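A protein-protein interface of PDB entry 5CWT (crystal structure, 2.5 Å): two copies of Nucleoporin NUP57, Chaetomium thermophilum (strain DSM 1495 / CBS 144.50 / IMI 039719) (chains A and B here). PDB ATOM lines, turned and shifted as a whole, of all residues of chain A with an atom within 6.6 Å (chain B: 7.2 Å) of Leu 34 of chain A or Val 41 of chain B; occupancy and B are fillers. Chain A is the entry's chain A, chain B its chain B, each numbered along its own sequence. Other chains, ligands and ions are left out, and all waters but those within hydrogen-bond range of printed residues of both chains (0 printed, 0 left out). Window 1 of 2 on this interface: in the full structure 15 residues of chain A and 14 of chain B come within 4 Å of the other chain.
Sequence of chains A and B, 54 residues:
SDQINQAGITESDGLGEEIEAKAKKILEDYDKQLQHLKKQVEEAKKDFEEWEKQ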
ATOM      1  N   ASP A  29      -7.576   2.803   8.347  1.00  0.00           N
ATOM      2  CA  ASP A  29      -7.756   4.215   8.668  1.00  0.00           C
ATOM      3  C   ASP A  29      -8.069   5.002   7.402  1.00  0.00           C
ATOM      4  O   ASP A  29      -8.935   5.877   7.395  1.00  0.00           O
ATOM      5  CB  ASP A  29      -6.497   4.783   9.328  1.00  0.00           C
ATOM      6  CG  ASP A  29      -6.175   4.112  10.650  1.00  0.00           C
ATOM      7  OD1 ASP A  29      -7.080   3.482  11.236  1.00  0.00           O
ATOM      8  OD2 ASP A  29      -5.016   4.220  11.104  1.00  0.00           O
ATOM      9  N   TYR A  30      -7.347   4.679   6.334  1.00  0.00           N
ATOM     10  CA  TYR A  30      -7.544   5.311   5.038  1.00  0.00           C
ATOM     11  C   TYR A  30      -8.977   5.098   4.562  1.00  0.00           C
ATOM     12  O   TYR A  30      -9.648   6.040   4.146  1.00  0.00           O
ATOM     13  CB  TYR A  30      -6.543   4.727   4.039  1.00  0.00           C
ATOM     14  CG  TYR A  30      -6.667   5.232   2.619  1.00  0.00           C
ATOM     15  CD1 TYR A  30      -6.745   6.591   2.341  1.00  0.00           C
ATOM     16  CD2 TYR A  30      -6.669   4.345   1.551  1.00  0.00           C
ATOM     17  CE1 TYR A  30      -6.844   7.048   1.039  1.00  0.00           C
ATOM     18  CE2 TYR A  30      -6.766   4.790   0.250  1.00  0.00           C
ATOM     19  CZ  TYR A  30      -6.851   6.139  -0.003  1.00  0.00           C
ATOM     20  OH  TYR A  30      -6.947   6.573  -1.303  1.00  0.00           O
ATOM     21  N   ASP A  31      -9.446   3.858   4.647  1.00  0.00           N
ATOM     22  CA  ASP A  31     -10.806   3.522   4.242  1.00  0.00           C
ATOM     23  C   ASP A  31     -11.838   4.269   5.080  1.00  0.00           C
ATOM     24  O   ASP A  31     -12.862   4.712   4.564  1.00  0.00           O
ATOM     25  CB  ASP A  31     -11.044   2.018   4.374  1.00  0.00           C
ATOM     26  CG  ASP A  31     -12.422   1.604   3.898  1.00  0.00           C
ATOM     27  OD1 ASP A  31     -12.820   2.022   2.791  1.00  0.00           O
ATOM     28  OD2 ASP A  31     -13.112   0.867   4.633  1.00  0.00           O
ATOM     29  N   LYS A  32     -11.567   4.394   6.376  1.00  0.00           N
ATOM     30  CA  LYS A  32     -12.468   5.087   7.290  1.00  0.00           C
ATOM     31  C   LYS A  32     -12.708   6.519   6.839  1.00  0.00           C
ATOM     32  O   LYS A  32     -13.850   6.969   6.765  1.00  0.00           O
ATOM     33  CB  LYS A  32     -11.893   5.084   8.708  1.00  0.00           C
ATOM     34  CG  LYS A  32     -12.444   3.980   9.588  1.00  0.00           C
ATOM     35  CD  LYS A  32     -13.813   4.347  10.138  1.00  0.00           C
ATOM     36  CE  LYS A  32     -14.761   3.162  10.117  1.00  0.00           C
ATOM     37  NZ  LYS A  32     -15.267   2.889   8.741  1.00  0.00           N
ATOM     38  N   GLN A  33     -11.626   7.226   6.534  1.00  0.00           N
ATOM     39  CA  GLN A  33     -11.710   8.609   6.084  1.00  0.00           C
ATOM     40  C   GLN A  33     -12.511   8.729   4.791  1.00  0.00           C
ATOM     41  O   GLN A  33     -13.298   9.662   4.629  1.00  0.00           O
ATOM     42  CB  GLN A  33     -10.306   9.188   5.883  1.00  0.00           C
ATOM     43  CG  GLN A  33      -9.470   9.252   7.156  1.00  0.00           C
ATOM     44  CD  GLN A  33     -10.047  10.202   8.189  1.00  0.00           C
ATOM     45  OE1 GLN A  33     -10.847  11.081   7.865  1.00  0.00           O
ATOM     46  NE2 GLN A  33      -9.644  10.028   9.441  1.00  0.00           N
ATOM     47  N   LEU A  34     -12.312   7.783   3.877  1.00  0.00           N
ATOM     48  CA  LEU A  34     -13.005   7.803   2.591  1.00  0.00           C
ATOM     49  C   LEU A  34     -14.497   7.560   2.773  1.00  0.00           C
ATOM     50  O   LEU A  34     -15.324   8.245   2.174  1.00  0.00           O
ATOM     51  CB  LEU A  34     -12.424   6.748   1.647  1.00  0.00           C
ATOM     52  CG  LEU A  34     -10.977   6.937   1.184  1.00  0.00           C
ATOM     53  CD1 LEU A  34     -10.510   5.707   0.423  1.00  0.00           C
ATOM     54  CD2 LEU A  34     -10.822   8.178   0.324  1.00  0.00           C
ATOM     55  N   GLN A  35     -14.837   6.579   3.605  1.00  0.00           N
ATOM     56  CA  GLN A  35     -16.232   6.230   3.848  1.00  0.00           C
ATOM     57  C   GLN A  35     -16.973   7.371   4.535  1.00  0.00           C
ATOM     58  O   GLN A  35     -18.149   7.606   4.265  1.00  0.00           O
ATOM     59  CB  GLN A  35     -16.327   4.963   4.699  1.00  0.00           C
ATOM     60  CG  GLN A  35     -15.896   3.697   3.975  1.00  0.00           C
ATOM     61  CD  GLN A  35     -16.782   3.370   2.789  1.00  0.00           C
ATOM     62  OE1 GLN A  35     -17.943   3.772   2.737  1.00  0.00           O
ATOM     63  NE2 GLN A  35     -16.233   2.641   1.825  1.00  0.00           N
ATOM     64  N   HIS A  36     -16.280   8.075   5.422  1.00  0.00           N
ATOM     65  CA  HIS A  36     -16.876   9.197   6.133  1.00  0.00           C
ATOM     66  C   HIS A  36     -17.051  10.379   5.191  1.00  0.00           C
ATOM     67  O   HIS A  36     -18.099  11.022   5.179  1.00  0.00           O
ATOM     68  CB  HIS A  36     -16.009   9.601   7.326  1.00  0.00           C
ATOM     69  CG  HIS A  36     -16.604  10.694   8.160  1.00  0.00           C
ATOM     70  ND1 HIS A  36     -15.969  11.897   8.374  1.00  0.00           N
ATOM     71  CD2 HIS A  36     -17.781  10.763   8.827  1.00  0.00           C
ATOM     72  CE1 HIS A  36     -16.726  12.662   9.142  1.00  0.00           C
ATOM     73  NE2 HIS A  36     -17.830  11.997   9.430  1.00  0.00           N
ATOM     74  N   LEU A  37     -16.021  10.662   4.401  1.00  0.00           N
ATOM     75  CA  LEU A  37     -16.086  11.753   3.440  1.00  0.00           C
ATOM     76  C   LEU A  37     -17.146  11.459   2.391  1.00  0.00           C
ATOM     77  O   LEU A  37     -17.873  12.354   1.966  1.00  0.00           O
ATOM     78  CB  LEU A  37     -14.730  11.970   2.767  1.00  0.00           C
ATOM     79  CG  LEU A  37     -14.694  13.036   1.668  1.00  0.00           C
ATOM     80  CD1 LEU A  37     -15.114  14.397   2.207  1.00  0.00           C
ATOM     81  CD2 LEU A  37     -13.312  13.115   1.052  1.00  0.00           C
ATOM     82  N   LYS A  38     -17.236  10.199   1.982  1.00  0.00           N
ATOM     83  CA  LYS A  38     -18.222   9.785   0.994  1.00  0.00           C
ATOM     84  C   LYS A  38     -19.634  10.051   1.497  1.00  0.00           C
ATOM     85  O   LYS A  38     -20.516  10.431   0.729  1.00  0.00           O
ATOM     86  CB  LYS A  38     -18.062   8.301   0.669  1.00  0.00           C
ATOM     87  CG  LYS A  38     -19.108   7.774  -0.294  1.00  0.00           C
ATOM     88  CD  LYS A  38     -18.739   6.404  -0.831  1.00  0.00           C
ATOM     89  CE  LYS A  38     -18.857   5.323   0.233  1.00  0.00           C
ATOM     90  NZ  LYS A  38     -20.272   5.063   0.617  1.00  0.00           N
ATOM     91  N   LYS A  39     -19.839   9.850   2.795  1.00  0.00           N
ATOM     92  CA  LYS A  39     -21.133  10.102   3.413  1.00  0.00           C
ATOM     93  C   LYS A  39     -21.469  11.590   3.360  1.00  0.00           C
ATOM     94  O   LYS A  39     -22.623  11.966   3.162  1.00  0.00           O
ATOM     95  CB  LYS A  39     -21.132   9.608   4.861  1.00  0.00           C
ATOM     96  CG  LYS A  39     -22.446   9.822   5.597  1.00  0.00           C
ATOM     97  CD  LYS A  39     -22.473   9.084   6.930  1.00  0.00           C
ATOM     98  CE  LYS A  39     -21.395   9.584   7.881  1.00  0.00           C
ATOM     99  NZ  LYS A  39     -21.457   8.901   9.203  1.00  0.00           N
ATOM    100  N   GLN B  35     -18.012   8.772  -7.304  1.00  0.00           N
ATOM    101  CA  GLN B  35     -17.462   7.649  -8.052  1.00  0.00           C
ATOM    102  C   GLN B  35     -15.966   7.520  -7.803  1.00  0.00           C
ATOM    103  O   GLN B  35     -15.443   6.414  -7.665  1.00  0.00           O
ATOM    104  CB  GLN B  35     -17.732   7.809  -9.550  1.00  0.00           C
ATOM    105  CG  GLN B  35     -19.207   7.761  -9.927  1.00  0.00           C
ATOM    106  CD  GLN B  35     -19.883   6.472  -9.503  1.00  0.00           C
ATOM    107  OE1 GLN B  35     -19.268   5.405  -9.500  1.00  0.00           O
ATOM    108  NE2 GLN B  35     -21.158   6.565  -9.137  1.00  0.00           N
ATOM    109  N   HIS B  36     -15.282   8.656  -7.733  1.00  0.00           N
ATOM    110  CA  HIS B  36     -13.843   8.654  -7.530  1.00  0.00           C
ATOM    111  C   HIS B  36     -13.473   8.196  -6.118  1.00  0.00           C
ATOM    112  O   HIS B  36     -12.362   7.719  -5.886  1.00  0.00           O
ATOM    113  CB  HIS B  36     -13.272  10.042  -7.802  1.00  0.00           C
ATOM    114  CG  HIS B  36     -11.793  10.123  -7.621  1.00  0.00           C
ATOM    115  ND1 HIS B  36     -10.910   9.315  -8.308  1.00  0.00           N
ATOM    116  CD2 HIS B  36     -11.039  10.902  -6.816  1.00  0.00           C
ATOM    117  CE1 HIS B  36      -9.677   9.601  -7.936  1.00  0.00           C
ATOM    118  NE2 HIS B  36      -9.725  10.563  -7.032  1.00  0.00           N
ATOM    119  N   LEU B  37     -14.403   8.343  -5.179  1.00  0.00           N
ATOM    120  CA  LEU B  37     -14.182   7.877  -3.814  1.00  0.00           C
ATOM    121  C   LEU B  37     -14.386   6.368  -3.715  1.00  0.00           C
ATOM    122  O   LEU B  37     -13.582   5.672  -3.097  1.00  0.00           O
ATOM    123  CB  LEU B  37     -15.107   8.601  -2.835  1.00  0.00           C
ATOM    124  CG  LEU B  37     -14.719  10.043  -2.494  1.00  0.00           C
ATOM    125  CD1 LEU B  37     -15.846  10.735  -1.746  1.00  0.00           C
ATOM    126  CD2 LEU B  37     -13.434  10.095  -1.679  1.00  0.00           C
ATOM    127  N   LYS B  38     -15.459   5.865  -4.320  1.00  0.00           N
ATOM    128  CA  LYS B  38     -15.699   4.425  -4.355  1.00  0.00           C
ATOM    129  C   LYS B  38     -14.574   3.729  -5.111  1.00  0.00           C
ATOM    130  O   LYS B  38     -14.277   2.561  -4.863  1.00  0.00           O
ATOM    131  CB  LYS B  38     -17.046   4.106  -5.011  1.00  0.00           C
ATOM    132  CG  LYS B  38     -18.272   4.528  -4.205  1.00  0.00           C
ATOM    133  CD  LYS B  38     -18.295   3.937  -2.795  1.00  0.00           C
ATOM    134  CE  LYS B  38     -18.176   2.420  -2.786  1.00  0.00           C
ATOM    135  NZ  LYS B  38     -18.326   1.870  -1.407  1.00  0.00           N
ATOM    136  N   LYS B  39     -13.953   4.453  -6.034  1.00  0.00           N
ATOM    137  CA  LYS B  39     -12.786   3.949  -6.741  1.00  0.00           C
ATOM    138  C   LYS B  39     -11.648   3.725  -5.752  1.00  0.00           C
ATOM    139  O   LYS B  39     -11.053   2.649  -5.709  1.00  0.00           O
ATOM    140  CB  LYS B  39     -12.356   4.940  -7.823  1.00  0.00           C
ATOM    141  CG  LYS B  39     -11.139   4.512  -8.624  1.00  0.00           C
ATOM    142  CD  LYS B  39     -10.785   5.552  -9.673  1.00  0.00           C
ATOM    143  CE  LYS B  39      -9.608   5.108 -10.524  1.00  0.00           C
ATOM    144  NZ  LYS B  39      -9.298   6.090 -11.599  1.00  0.00           N
ATOM    145  N   GLN B  40     -11.358   4.748  -4.952  1.00  0.00           N
ATOM    146  CA  GLN B  40     -10.285   4.677  -3.966  1.00  0.00           C
ATOM    147  C   GLN B  40     -10.554   3.618  -2.905  1.00  0.00           C
ATOM    148  O   GLN B  40      -9.627   2.961  -2.431  1.00  0.00           O
ATOM    149  CB  GLN B  40     -10.096   6.030  -3.286  1.00  0.00           C
ATOM    150  CG  GLN B  40      -9.457   7.081  -4.158  1.00  0.00           C
ATOM    151  CD  GLN B  40      -9.354   8.414  -3.453  1.00  0.00           C
ATOM    152  OE1 GLN B  40      -8.351   8.713  -2.807  1.00  0.00           O
ATOM    153  NE2 GLN B  40     -10.402   9.219  -3.563  1.00  0.00           N
ATOM    154  N   VAL B  41     -11.818   3.465  -2.523  1.00  0.00           N
ATOM    155  CA  VAL B  41     -12.196   2.433  -1.564  1.00  0.00           C
ATOM    156  C   VAL B  41     -11.877   1.065  -2.148  1.00  0.00           C
ATOM    157  O   VAL B  41     -11.453   0.159  -1.432  1.00  0.00           O
ATOM    158  CB  VAL B  41     -13.696   2.507  -1.200  1.00  0.00           C
ATOM    159  CG1 VAL B  41     -14.125   1.288  -0.382  1.00  0.00           C
ATOM    160  CG2 VAL B  41     -13.992   3.776  -0.427  1.00  0.00           C
ATOM    161  N   GLU B  42     -12.081   0.920  -3.454  1.00  0.00           N
ATOM    162  CA  GLU B  42     -11.813  -0.343  -4.127  1.00  0.00           C
ATOM    163  C   GLU B  42     -10.310  -0.578  -4.243  1.00  0.00           C
ATOM    164  O   GLU B  42      -9.839  -1.706  -4.101  1.00  0.00           O
ATOM    165  CB  GLU B  42     -12.461  -0.365  -5.513  1.00  0.00           C
ATOM    166  CG  GLU B  42     -12.663  -1.765  -6.077  1.00  0.00           C
ATOM    167  CD  GLU B  42     -13.610  -2.608  -5.237  1.00  0.00           C
ATOM    168  OE1 GLU B  42     -14.394  -2.028  -4.454  1.00  0.00           O
ATOM    169  OE2 GLU B  42     -13.568  -3.851  -5.356  1.00  0.00           O
ATOM    170  N   GLU B  43      -9.562   0.491  -4.498  1.00  0.00           N
ATOM    171  CA  GLU B  43      -8.107   0.411  -4.535  1.00  0.00           C
ATOM    172  C   GLU B  43      -7.563   0.036  -3.162  1.00  0.00           C
ATOM    173  O   GLU B  43      -6.656  -0.787  -3.045  1.00  0.00           O
ATOM    174  CB  GLU B  43      -7.507   1.745  -4.979  1.00  0.00           C
ATOM    175  CG  GLU B  43      -7.771   2.095  -6.431  1.00  0.00           C
ATOM    176  CD  GLU B  43      -7.066   3.366  -6.862  1.00  0.00           C
ATOM    177  OE1 GLU B  43      -6.152   3.818  -6.140  1.00  0.00           O
ATOM    178  OE2 GLU B  43      -7.428   3.916  -7.923  1.00  0.00           O
ATOM    179  N   ALA B  44      -8.115   0.650  -2.121  1.00  0.00           N
ATOM    180  CA  ALA B  44      -7.700   0.345  -0.759  1.00  0.00           C
ATOM    181  C   ALA B  44      -8.052  -1.095  -0.415  1.00  0.00           C
ATOM    182  O   ALA B  44      -7.361  -1.740   0.373  1.00  0.00           O
ATOM    183  CB  ALA B  44      -8.358   1.300   0.223  1.00  0.00           C
ATOM    184  N   LYS B  45      -9.127  -1.595  -1.013  1.00  0.00           N
ATOM    185  CA  LYS B  45      -9.585  -2.950  -0.746  1.00  0.00           C
ATOM    186  C   LYS B  45      -8.620  -3.974  -1.334  1.00  0.00           C
ATOM    187  O   LYS B  45      -8.255  -4.943  -0.669  1.00  0.00           O
ATOM    188  CB  LYS B  45     -10.986  -3.157  -1.325  1.00  0.00           C
ATOM    189  CG  LYS B  45     -11.765  -4.283  -0.669  1.00  0.00           C
ATOM    190  CD  LYS B  45     -13.021  -3.764   0.021  1.00  0.00           C
ATOM    191  CE  LYS B  45     -14.125  -3.451  -0.979  1.00  0.00           C
ATOM    192  NZ  LYS B  45     -15.274  -2.747  -0.340  1.00  0.00           N
ATOM    193  N   LYS B  46      -8.200  -3.756  -2.578  1.00  0.00           N
ATOM    194  CA  LYS B  46      -7.318  -4.703  -3.252  1.00  0.00           C
ATOM    195  C   LYS B  46      -5.916  -4.681  -2.640  1.00  0.00           C
ATOM    196  O   LYS B  46      -5.223  -5.699  -2.630  1.00  0.00           O
ATOM    197  CB  LYS B  46      -7.270  -4.430  -4.763  1.00  0.00           C
ATOM    198  CG  LYS B  46      -6.328  -3.314  -5.197  1.00  0.00           C
ATOM    199  CD  LYS B  46      -6.476  -3.017  -6.685  1.00  0.00           C
ATOM    200  CE  LYS B  46      -5.640  -1.817  -7.108  1.00  0.00           C
ATOM    201  NZ  LYS B  46      -5.773  -1.514  -8.558  1.00  0.00           N
ATOM    202  N   ASP B  47      -5.503  -3.527  -2.127  1.00  0.00           N
ATOM    203  CA  ASP B  47      -4.229  -3.422  -1.423  1.00  0.00           C
ATOM    204  C   ASP B  47      -4.285  -4.196  -0.113  1.00  0.00           C
ATOM    205  O   ASP B  47      -3.317  -4.845   0.278  1.00  0.00           O
ATOM    206  CB  ASP B  47      -3.889  -1.961  -1.129  1.00  0.00           C
ATOM    207  CG  ASP B  47      -3.406  -1.213  -2.353  1.00  0.00           C
ATOM    208  OD1 ASP B  47      -2.703  -1.818  -3.189  1.00  0.00           O
ATOM    209  OD2 ASP B  47      -3.727  -0.013  -2.476  1.00  0.00           O
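OE1 of Gln 40 of chain B sits at hydrogen-bond distance from OH of Tyr 30 of chain A (3.0 Å).
The side-chain amide nitrogen (NE2) of Gln 40 of chain B lies within hydrogen-bond range of the backbone carbonyl oxygen (O) of His 36 of chain B (3.4 Å). NZ of Lys 38 of chain A sits close to OE1 of Gln 35 of chain A, at 3.4 Å.
Among the printed residues, merely in contact across the chains: Lys 38 of chain A with Lys 38 of chain B, Gln 35 of chain A with Val 41 of chain B, Asp 31 of chain A with Val 41 of chain B, Tyr 30 of chain A with Ala 44 of chain B, Leu 34 of chain A with Gln 40 of chain B, Lys 38 of chain A with Leu 37 of chain B, Leu 34 of chain A with Leu 37 of chain B, Leu 34 of chain A with Val 41 of chain B and Gln 35 of chain A with Lys 38 of chain B.
Val 41 of chain B touches just these residues of chain A: Asp 31 (3.5 Å), Leu 34 (3.9 Å) and Gln 35 (3.3 Å). Of the printed residues of chain B, Tyr 30 of chain A touches Gln 40 (3.0 Å) and Ala 44 (3.7 Å). Of the printed residues of chain A, Leu 37 of chain B touches Leu 34 (3.8 Å) and Lys 38 (3.7 Å). Printed residues of chain A within 4 Å of Lys 38 of chain B: Gln 35 (3.9 Å) and Lys 38 (3.2 Å). Of the printed residues of chain B, Gln 35 of chain A touches Lys 38 and Val 41. Printed residues of chain B within 4 Å of Asp 31 of chain A: Val 41 (3.5 Å). Lys 39 of chain A touches none of the printed residues of chain B. Glu 43 of chain B touches none of the printed residues of chain A. The nearest residue of chain B that does not touch Leu 34 of chain A is Ala 44 of chain B (4.9 Å). The nearest residue of chain A that does not touch Val 41 of chain B is Lys 38 of chain A (5.1 Å).
Printed residues of chain B that touch a printed residue of chain A: Leu 37, Lys 38, Gln 40, Val 41 and Ala 44. Along chain B the printed residues that touch a printed residue of chain A span positions 37 to 44. Printed residues of chain A that touch a printed residue of chain B: Tyr 30, Asp 31, Leu 34, Gln 35 and Lys 38.
Gln 35 of chain A touches Lys 38 of chain B, but with the chains exchanged Lys 38 of chain A does not touch Gln 35 of chain B (6.9 Å). Lys 38 of chain A touches Leu 37 of chain B, but with the chains exchanged Leu 37 of chain A does not touch Lys 38 of chain B (8.9 Å). Lys 38 of chain B touches its own counterpart, Lys 38 of chain A. Positions printed for both chains: 35, 36, 37, 38 and 39.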
